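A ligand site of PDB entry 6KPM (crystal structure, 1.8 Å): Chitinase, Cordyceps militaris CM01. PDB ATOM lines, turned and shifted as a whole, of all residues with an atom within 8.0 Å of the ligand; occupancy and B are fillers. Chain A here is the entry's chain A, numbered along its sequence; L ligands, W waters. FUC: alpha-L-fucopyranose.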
ATOM      1  N   ASP A 136     -20.797 -25.466  17.874  1.00  0.00           N
ATOM      2  CA  ASP A 136     -19.370 -25.052  18.006  1.00  0.00           C
ATOM      3  C   ASP A 136     -18.768 -24.934  16.594  1.00  0.00           C
ATOM      4  O   ASP A 136     -18.544 -25.992  15.935  1.00  0.00           O
ATOM      5  CB  ASP A 136     -18.665 -26.038  18.939  1.00  0.00           C
ATOM      6  CG  ASP A 136     -17.208 -25.728  19.229  1.00  0.00           C
ATOM      7  OD1 ASP A 136     -16.597 -24.905  18.474  1.00  0.00           O
ATOM      8  OD2 ASP A 136     -16.654 -26.368  20.205  1.00  0.00           O
ATOM      9  N   VAL A 137     -18.512 -23.708  16.168  1.00  0.00           N
ATOM     10  CA  VAL A 137     -18.000 -23.394  14.821  1.00  0.00           C
ATOM     11  C   VAL A 137     -16.533 -22.943  14.920  1.00  0.00           C
ATOM     12  O   VAL A 137     -16.303 -21.775  15.307  1.00  0.00           O
ATOM     13  CB  VAL A 137     -18.882 -22.373  14.115  1.00  0.00           C
ATOM     14  CG1 VAL A 137     -18.433 -22.142  12.694  1.00  0.00           C
ATOM     15  CG2 VAL A 137     -20.353 -22.773  14.234  1.00  0.00           C
ATOM     16  N   GLU A 138     -15.592 -23.809  14.528  1.00  0.00           N
ATOM     17  CA  GLU A 138     -14.132 -23.499  14.612  1.00  0.00           C
ATOM     18  C   GLU A 138     -13.466 -23.848  13.283  1.00  0.00           C
ATOM     19  O   GLU A 138     -12.249 -24.170  13.264  1.00  0.00           O
ATOM     20  CB  GLU A 138     -13.492 -24.283  15.755  1.00  0.00           C
ATOM     21  CG  GLU A 138     -14.000 -23.914  17.137  1.00  0.00           C
ATOM     22  CD  GLU A 138     -13.452 -24.734  18.329  1.00  0.00           C
ATOM     23  OE1 GLU A 138     -14.225 -25.577  18.831  1.00  0.00           O
ATOM     24  OE2 GLU A 138     -12.283 -24.479  18.823  1.00  0.00           O
ATOM     25  N   THR A 174     -17.958 -19.811  18.759  1.00  0.00           N
ATOM     26  CA  THR A 174     -17.013 -19.753  17.641  1.00  0.00           C
ATOM     27  C   THR A 174     -15.674 -19.140  18.115  1.00  0.00           C
ATOM     28  O   THR A 174     -15.703 -18.342  19.040  1.00  0.00           O
ATOM     29  CB  THR A 174     -17.626 -18.991  16.452  1.00  0.00           C
ATOM     30  OG1 THR A 174     -16.767 -19.123  15.319  1.00  0.00           O
ATOM     31  CG2 THR A 174     -17.895 -17.530  16.750  1.00  0.00           C
ATOM     32  N   ASN A 175     -14.621 -19.513  17.425  1.00  0.00           N
ATOM     33  CA  ASN A 175     -13.299 -18.847  17.567  1.00  0.00           C
ATOM     34  C   ASN A 175     -13.034 -17.971  16.368  1.00  0.00           C
ATOM     35  O   ASN A 175     -11.953 -17.350  16.320  1.00  0.00           O
ATOM     36  CB  ASN A 175     -12.199 -19.875  17.807  1.00  0.00           C
ATOM     37  CG  ASN A 175     -11.970 -20.779  16.627  1.00  0.00           C
ATOM     38  OD1 ASN A 175     -12.739 -20.765  15.666  1.00  0.00           O
ATOM     39  ND2 ASN A 175     -10.911 -21.565  16.700  1.00  0.00           N
ATOM     40  N   MET A 176     -14.032 -17.768  15.492  1.00  0.00           N
ATOM     41  CA  MET A 176     -13.866 -16.931  14.284  1.00  0.00           C
ATOM     42  C   MET A 176     -14.707 -15.656  14.467  1.00  0.00           C
ATOM     43  O   MET A 176     -15.243 -15.483  15.521  1.00  0.00           O
ATOM     44  CB  MET A 176     -14.240 -17.738  13.041  1.00  0.00           C
ATOM     45  CG  MET A 176     -13.184 -18.813  12.744  1.00  0.00           C
ATOM     46  SD  MET A 176     -13.851 -20.129  11.637  1.00  0.00           S
ATOM     47  CE  MET A 176     -13.735 -19.269  10.073  1.00  0.00           C
ATOM     48  N   ILE A 195     -17.946 -16.074  21.950  1.00  0.00           N
ATOM     49  CA  ILE A 195     -16.628 -15.999  21.289  1.00  0.00           C
ATOM     50  C   ILE A 195     -15.581 -16.642  22.194  1.00  0.00           C
ATOM     51  O   ILE A 195     -15.293 -16.063  23.246  1.00  0.00           O
ATOM     52  CB  ILE A 195     -16.252 -14.561  20.951  1.00  0.00           C
ATOM     53  CG1 ILE A 195     -17.406 -13.783  20.304  1.00  0.00           C
ATOM     54  CG2 ILE A 195     -15.064 -14.586  20.051  1.00  0.00           C
ATOM     55  CD1 ILE A 195     -18.062 -14.504  19.102  1.00  0.00           C
ATOM     56  N   GLN A 196     -15.036 -17.765  21.754  1.00  0.00           N
ATOM     57  CA  GLN A 196     -13.851 -18.446  22.336  1.00  0.00           C
ATOM     58  C   GLN A 196     -12.697 -17.459  22.241  1.00  0.00           C
ATOM     59  O   GLN A 196     -12.290 -17.122  21.117  1.00  0.00           O
ATOM     60  CB  GLN A 196     -13.569 -19.741  21.574  1.00  0.00           C
ATOM     61  CG  GLN A 196     -14.720 -20.723  21.590  1.00  0.00           C
ATOM     62  CD  GLN A 196     -14.486 -21.829  20.592  1.00  0.00           C
ATOM     63  OE1 GLN A 196     -13.339 -22.078  20.206  1.00  0.00           O
ATOM     64  NE2 GLN A 196     -15.543 -22.495  20.139  1.00  0.00           N
ATOM     65  N   SER A 197     -12.257 -16.958  23.379  1.00  0.00           N
ATOM     66  CA  SER A 197     -11.238 -15.882  23.414  1.00  0.00           C
ATOM     67  C   SER A 197     -10.060 -16.297  24.309  1.00  0.00           C
ATOM     68  O   SER A 197      -9.482 -15.428  25.044  1.00  0.00           O
ATOM     69  CB  SER A 197     -11.902 -14.624  23.904  1.00  0.00           C
ATOM     70  OG  SER A 197     -13.037 -14.265  23.117  1.00  0.00           O
ATOM     71  N   TYR A 198      -9.787 -17.591  24.359  1.00  0.00           N
ATOM     72  CA  TYR A 198      -8.756 -18.132  25.286  1.00  0.00           C
ATOM     73  C   TYR A 198      -7.416 -17.513  24.905  1.00  0.00           C
ATOM     74  O   TYR A 198      -7.031 -17.429  23.705  1.00  0.00           O
ATOM     75  CB  TYR A 198      -8.750 -19.675  25.275  1.00  0.00           C
ATOM     76  CG  TYR A 198     -10.107 -20.337  25.186  1.00  0.00           C
ATOM     77  CD1 TYR A 198     -11.248 -19.760  25.734  1.00  0.00           C
ATOM     78  CD2 TYR A 198     -10.241 -21.561  24.521  1.00  0.00           C
ATOM     79  CE1 TYR A 198     -12.490 -20.375  25.642  1.00  0.00           C
ATOM     80  CE2 TYR A 198     -11.489 -22.176  24.421  1.00  0.00           C
ATOM     81  CZ  TYR A 198     -12.614 -21.569  24.955  1.00  0.00           C
ATOM     82  OH  TYR A 198     -13.856 -22.136  24.811  1.00  0.00           O
ATOM     83  N   GLY A 199      -6.694 -16.994  25.896  1.00  0.00           N
ATOM     84  CA  GLY A 199      -5.330 -16.487  25.666  1.00  0.00           C
ATOM     85  C   GLY A 199      -5.272 -15.187  24.871  1.00  0.00           C
ATOM     86  O   GLY A 199      -4.190 -14.790  24.549  1.00  0.00           O
ATOM     87  N   ARG A 200      -6.363 -14.459  24.647  1.00  0.00           N
ATOM     88  CA  ARG A 200      -6.338 -13.346  23.693  1.00  0.00           C
ATOM     89  C   ARG A 200      -6.020 -12.042  24.439  1.00  0.00           C
ATOM     90  O   ARG A 200      -6.261 -11.964  25.697  1.00  0.00           O
ATOM     91  CB  ARG A 200      -7.692 -13.259  22.987  1.00  0.00           C
ATOM     92  CG  ARG A 200      -7.951 -14.443  22.064  1.00  0.00           C
ATOM     93  CD  ARG A 200      -9.063 -14.103  21.081  1.00  0.00           C
ATOM     94  NE  ARG A 200      -9.384 -15.194  20.202  1.00  0.00           N
ATOM     95  CZ  ARG A 200     -10.376 -15.182  19.315  1.00  0.00           C
ATOM     96  NH1 ARG A 200     -11.123 -14.106  19.163  1.00  0.00           N
ATOM     97  NH2 ARG A 200     -10.558 -16.230  18.529  1.00  0.00           N
ATOM     98  N   SER A 201      -5.680 -11.036  23.635  1.00  0.00           N
ATOM     99  CA  SER A 201      -5.379  -9.665  24.111  1.00  0.00           C
ATOM    100  C   SER A 201      -6.672  -8.963  24.507  1.00  0.00           C
ATOM    101  O   SER A 201      -7.608  -8.939  23.690  1.00  0.00           O
ATOM    102  CB  SER A 201      -4.632  -8.911  23.033  1.00  0.00           C
ATOM    103  OG  SER A 201      -4.481  -7.554  23.386  1.00  0.00           O
ATOM    104  N   GLY A 224     -15.390 -15.788  26.079  1.00  0.00           N
ATOM    105  CA  GLY A 224     -15.044 -16.964  26.894  1.00  0.00           C
ATOM    106  C   GLY A 224     -13.552 -17.022  27.223  1.00  0.00           C
ATOM    107  O   GLY A 224     -12.707 -16.709  26.365  1.00  0.00           O
ATOM    108  N   PHE A 225     -13.266 -17.446  28.441  1.00  0.00           N
ATOM    109  CA  PHE A 225     -11.895 -17.839  28.851  1.00  0.00           C
ATOM    110  C   PHE A 225     -11.920 -19.348  29.105  1.00  0.00           C
ATOM    111  O   PHE A 225     -13.002 -19.984  29.232  1.00  0.00           O
ATOM    112  CB  PHE A 225     -11.470 -17.042  30.092  1.00  0.00           C
ATOM    113  CG  PHE A 225     -12.204 -17.448  31.325  1.00  0.00           C
ATOM    114  CD1 PHE A 225     -13.452 -16.911  31.627  1.00  0.00           C
ATOM    115  CD2 PHE A 225     -11.690 -18.404  32.191  1.00  0.00           C
ATOM    116  CE1 PHE A 225     -14.133 -17.292  32.779  1.00  0.00           C
ATOM    117  CE2 PHE A 225     -12.370 -18.786  33.329  1.00  0.00           C
ATOM    118  CZ  PHE A 225     -13.597 -18.219  33.640  1.00  0.00           C
ATOM    119  N   SER A 226     -10.739 -19.942  29.240  1.00  0.00           N
ATOM    120  CA  SER A 226     -10.614 -21.379  29.565  1.00  0.00           C
ATOM    121  C   SER A 226      -9.990 -21.560  30.953  1.00  0.00           C
ATOM    122  O   SER A 226      -9.055 -20.796  31.308  1.00  0.00           O
ATOM    123  CB  SER A 226      -9.818 -22.105  28.542  1.00  0.00           C
ATOM    124  OG  SER A 226      -9.783 -23.482  28.847  1.00  0.00           O
ATOM    125  N   THR A 233      -3.632 -27.151  26.662  1.00  0.00           N
ATOM    126  CA  THR A 233      -2.992 -25.878  26.300  1.00  0.00           C
ATOM    127  C   THR A 233      -2.870 -24.967  27.521  1.00  0.00           C
ATOM    128  O   THR A 233      -3.820 -24.890  28.332  1.00  0.00           O
ATOM    129  CB  THR A 233      -3.772 -25.150  25.193  1.00  0.00           C
ATOM    130  OG1 THR A 233      -3.809 -26.056  24.095  1.00  0.00           O
ATOM    131  CG2 THR A 233      -3.132 -23.839  24.779  1.00  0.00           C
ATOM    132  N   TRP A 235      -3.284 -21.648  28.246  1.00  0.00           N
ATOM    133  CA  TRP A 235      -3.827 -20.364  27.722  1.00  0.00           C
ATOM    134  C   TRP A 235      -3.466 -19.230  28.682  1.00  0.00           C
ATOM    135  O   TRP A 235      -3.443 -18.102  28.226  1.00  0.00           O
ATOM    136  CB  TRP A 235      -5.353 -20.465  27.605  1.00  0.00           C
ATOM    137  CG  TRP A 235      -5.813 -21.392  26.538  1.00  0.00           C
ATOM    138  CD1 TRP A 235      -6.505 -22.542  26.745  1.00  0.00           C
ATOM    139  CD2 TRP A 235      -5.645 -21.246  25.124  1.00  0.00           C
ATOM    140  NE1 TRP A 235      -6.790 -23.118  25.551  1.00  0.00           N
ATOM    141  CE2 TRP A 235      -6.257 -22.377  24.541  1.00  0.00           C
ATOM    142  CE3 TRP A 235      -5.039 -20.306  24.304  1.00  0.00           C
ATOM    143  CZ2 TRP A 235      -6.317 -22.546  23.167  1.00  0.00           C
ATOM    144  CZ3 TRP A 235      -5.058 -20.496  22.936  1.00  0.00           C
ATOM    145  CH2 TRP A 235      -5.717 -21.594  22.389  1.00  0.00           C
ATOM    146  N   ASP A 237      -5.381 -18.029  31.196  1.00  0.00           N
ATOM    147  CA  ASP A 237      -6.548 -17.156  31.447  1.00  0.00           C
ATOM    148  C   ASP A 237      -6.844 -17.035  32.939  1.00  0.00           C
ATOM    149  O   ASP A 237      -7.639 -16.152  33.305  1.00  0.00           O
ATOM    150  CB  ASP A 237      -7.793 -17.692  30.730  1.00  0.00           C
ATOM    151  CG  ASP A 237      -7.694 -17.710  29.224  1.00  0.00           C
ATOM    152  OD1 ASP A 237      -6.753 -17.092  28.675  1.00  0.00           O
ATOM    153  OD2 ASP A 237      -8.559 -18.388  28.595  1.00  0.00           O
ATOM    154  N   ARG A 246      -6.828 -12.810  33.125  1.00  0.00           N
ATOM    155  CA  ARG A 246      -7.619 -12.569  31.893  1.00  0.00           C
ATOM    156  C   ARG A 246      -9.107 -12.810  32.173  1.00  0.00           C
ATOM    157  O   ARG A 246      -9.921 -11.958  31.725  1.00  0.00           O
ATOM    158  CB  ARG A 246      -7.100 -13.427  30.737  1.00  0.00           C
ATOM    159  CG  ARG A 246      -7.811 -13.121  29.425  1.00  0.00           C
ATOM    160  CD  ARG A 246      -7.296 -13.977  28.312  1.00  0.00           C
ATOM    161  NE  ARG A 246      -6.008 -13.510  27.876  1.00  0.00           N
ATOM    162  CZ  ARG A 246      -4.828 -14.014  28.212  1.00  0.00           C
ATOM    163  NH1 ARG A 246      -4.717 -15.078  28.980  1.00  0.00           N
ATOM    164  NH2 ARG A 246      -3.761 -13.425  27.729  1.00  0.00           N
ATOM    165  N   TYR A 250     -12.013 -10.061  31.522  1.00  0.00           N
ATOM    166  CA  TYR A 250     -13.192 -10.384  30.680  1.00  0.00           C
ATOM    167  C   TYR A 250     -14.495 -10.074  31.431  1.00  0.00           C
ATOM    168  O   TYR A 250     -15.398  -9.490  30.809  1.00  0.00           O
ATOM    169  CB  TYR A 250     -13.187 -11.840  30.209  1.00  0.00           C
ATOM    170  CG  TYR A 250     -12.214 -12.142  29.120  1.00  0.00           C
ATOM    171  CD1 TYR A 250     -11.289 -11.229  28.660  1.00  0.00           C
ATOM    172  CD2 TYR A 250     -12.227 -13.394  28.514  1.00  0.00           C
ATOM    173  CE1 TYR A 250     -10.408 -11.496  27.630  1.00  0.00           C
ATOM    174  CE2 TYR A 250     -11.343 -13.700  27.508  1.00  0.00           C
ATOM    175  CZ  TYR A 250     -10.428 -12.766  27.081  1.00  0.00           C
ATOM    176  OH  TYR A 250      -9.585 -13.031  26.068  1.00  0.00           O
ATOM    177  N   PHE A 264     -18.353 -16.757  29.489  1.00  0.00           N
ATOM    178  CA  PHE A 264     -18.403 -18.207  29.723  1.00  0.00           C
ATOM    179  C   PHE A 264     -16.991 -18.736  30.017  1.00  0.00           C
ATOM    180  O   PHE A 264     -16.015 -18.131  29.643  1.00  0.00           O
ATOM    181  CB  PHE A 264     -18.996 -18.939  28.522  1.00  0.00           C
ATOM    182  CG  PHE A 264     -18.203 -18.906  27.245  1.00  0.00           C
ATOM    183  CD1 PHE A 264     -18.342 -17.858  26.347  1.00  0.00           C
ATOM    184  CD2 PHE A 264     -17.368 -19.970  26.893  1.00  0.00           C
ATOM    185  CE1 PHE A 264     -17.685 -17.871  25.127  1.00  0.00           C
ATOM    186  CE2 PHE A 264     -16.718 -19.972  25.665  1.00  0.00           C
ATOM    187  CZ  PHE A 264     -16.866 -18.923  24.787  1.00  0.00           C
ATOM    188  N   TYR A 266     -14.669 -22.272  29.385  1.00  0.00           N
ATOM    189  CA  TYR A 266     -14.397 -23.643  28.890  1.00  0.00           C
ATOM    190  C   TYR A 266     -13.808 -24.466  30.036  1.00  0.00           C
ATOM    191  O   TYR A 266     -12.977 -23.930  30.826  1.00  0.00           O
ATOM    192  CB  TYR A 266     -13.496 -23.641  27.656  1.00  0.00           C
ATOM    193  CG  TYR A 266     -13.479 -25.032  27.082  1.00  0.00           C
ATOM    194  CD1 TYR A 266     -14.621 -25.563  26.512  1.00  0.00           C
ATOM    195  CD2 TYR A 266     -12.399 -25.882  27.268  1.00  0.00           C
ATOM    196  CE1 TYR A 266     -14.675 -26.876  26.068  1.00  0.00           C
ATOM    197  CE2 TYR A 266     -12.414 -27.197  26.793  1.00  0.00           C
ATOM    198  CZ  TYR A 266     -13.556 -27.681  26.171  1.00  0.00           C
ATOM    199  OH  TYR A 266     -13.621 -28.982  25.761  1.00  0.00           O
HETATM  200  C1  FUC L   1      -9.987 -20.933  20.383  1.00  0.00           C
HETATM  201  C2  FUC L   1      -9.771 -19.508  20.911  1.00  0.00           C
HETATM  202  C3  FUC L   1      -8.294 -19.024  20.874  1.00  0.00           C
HETATM  203  C4  FUC L   1      -7.762 -19.263  19.480  1.00  0.00           C
HETATM  204  C5  FUC L   1      -8.020 -20.712  19.063  1.00  0.00           C
HETATM  205  C6  FUC L   1      -7.590 -20.922  17.634  1.00  0.00           C
HETATM  206  O1  FUC L   1      -9.431 -21.890  21.254  1.00  0.00           O
HETATM  207  O2  FUC L   1     -10.292 -19.562  22.243  1.00  0.00           O
HETATM  208  O3  FUC L   1      -8.261 -17.640  21.318  1.00  0.00           O
HETATM  209  O4  FUC L   1      -8.444 -18.386  18.584  1.00  0.00           O
HETATM  210  O5  FUC L   1      -9.415 -21.095  19.147  1.00  0.00           O
HETATM  211  O   HOH W   1     -10.386 -24.353  21.336  1.00  0.00           O
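The backbone carbonyl oxygen (O) of Gln 196 lies close to an oxygen (O2) of the ligand, at 3.3 Å.
An oxygen (O2) of the ligand sits at hydrogen-bond distance from the backbone NH of Ser 197 (3.5 Å).
The backbone NH (N) of Tyr 198 lies within hydrogen-bond range of an oxygen (O2) of the ligand, 2.9 Å away.
O5 of the ligand lies within hydrogen-bond range of ND2 of Asn 175, at 2.9 Å.
O of Tyr 198 lies within hydrogen-bond range of O3 of the ligand, at 2.7 Å.
NE of Arg 200 is in hydrogen-bond range of O3 of the ligand (2.9 Å).
The backbone carbonyl oxygen (O) of Ser 197 lies within hydrogen-bond range of the side-chain hydroxyl (OH) of Tyr 250.
The backbone carbonyl oxygen (O) of Gln 196 is in hydrogen-bond range of the guanidinium group (NH2) of Arg 200.
N of Gln 196 is in hydrogen-bond range of O of Thr 174 (2.9 Å).
O of Asn 175 sits at hydrogen-bond distance from NH2 of Arg 200.
The side-chain carboxylate (OE2) of Glu 138 lies close to the side-chain amide oxygen (OE1) of Gln 196 (3.0 Å).
O of Trp 235 lies within hydrogen-bond range of NH1 of Arg 246, 3.4 Å away.
The side-chain hydroxyl (OG) of Ser 197 is in hydrogen-bond range of the backbone carbonyl oxygen (O) of Ile 195, at 2.9 Å.
The side-chain carboxylate of Asp 136 sits at hydrogen-bond distance from the side-chain amide nitrogen of Gln 196 (3.1 Å).
Residues that only touch the ligand: Trp 235.
Hydrophobic or aromatic side chains that line the ligand: Tyr 198 and Trp 235.
The nearest printed residue that does not touch the ligand is Glu 138 (4.4 Å).
Water W1 lies within hydrogen-bond range of an oxygen (O1) of the ligand (2.6 Å) and the side-chain carboxylate of Glu 138 (3.2 Å).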
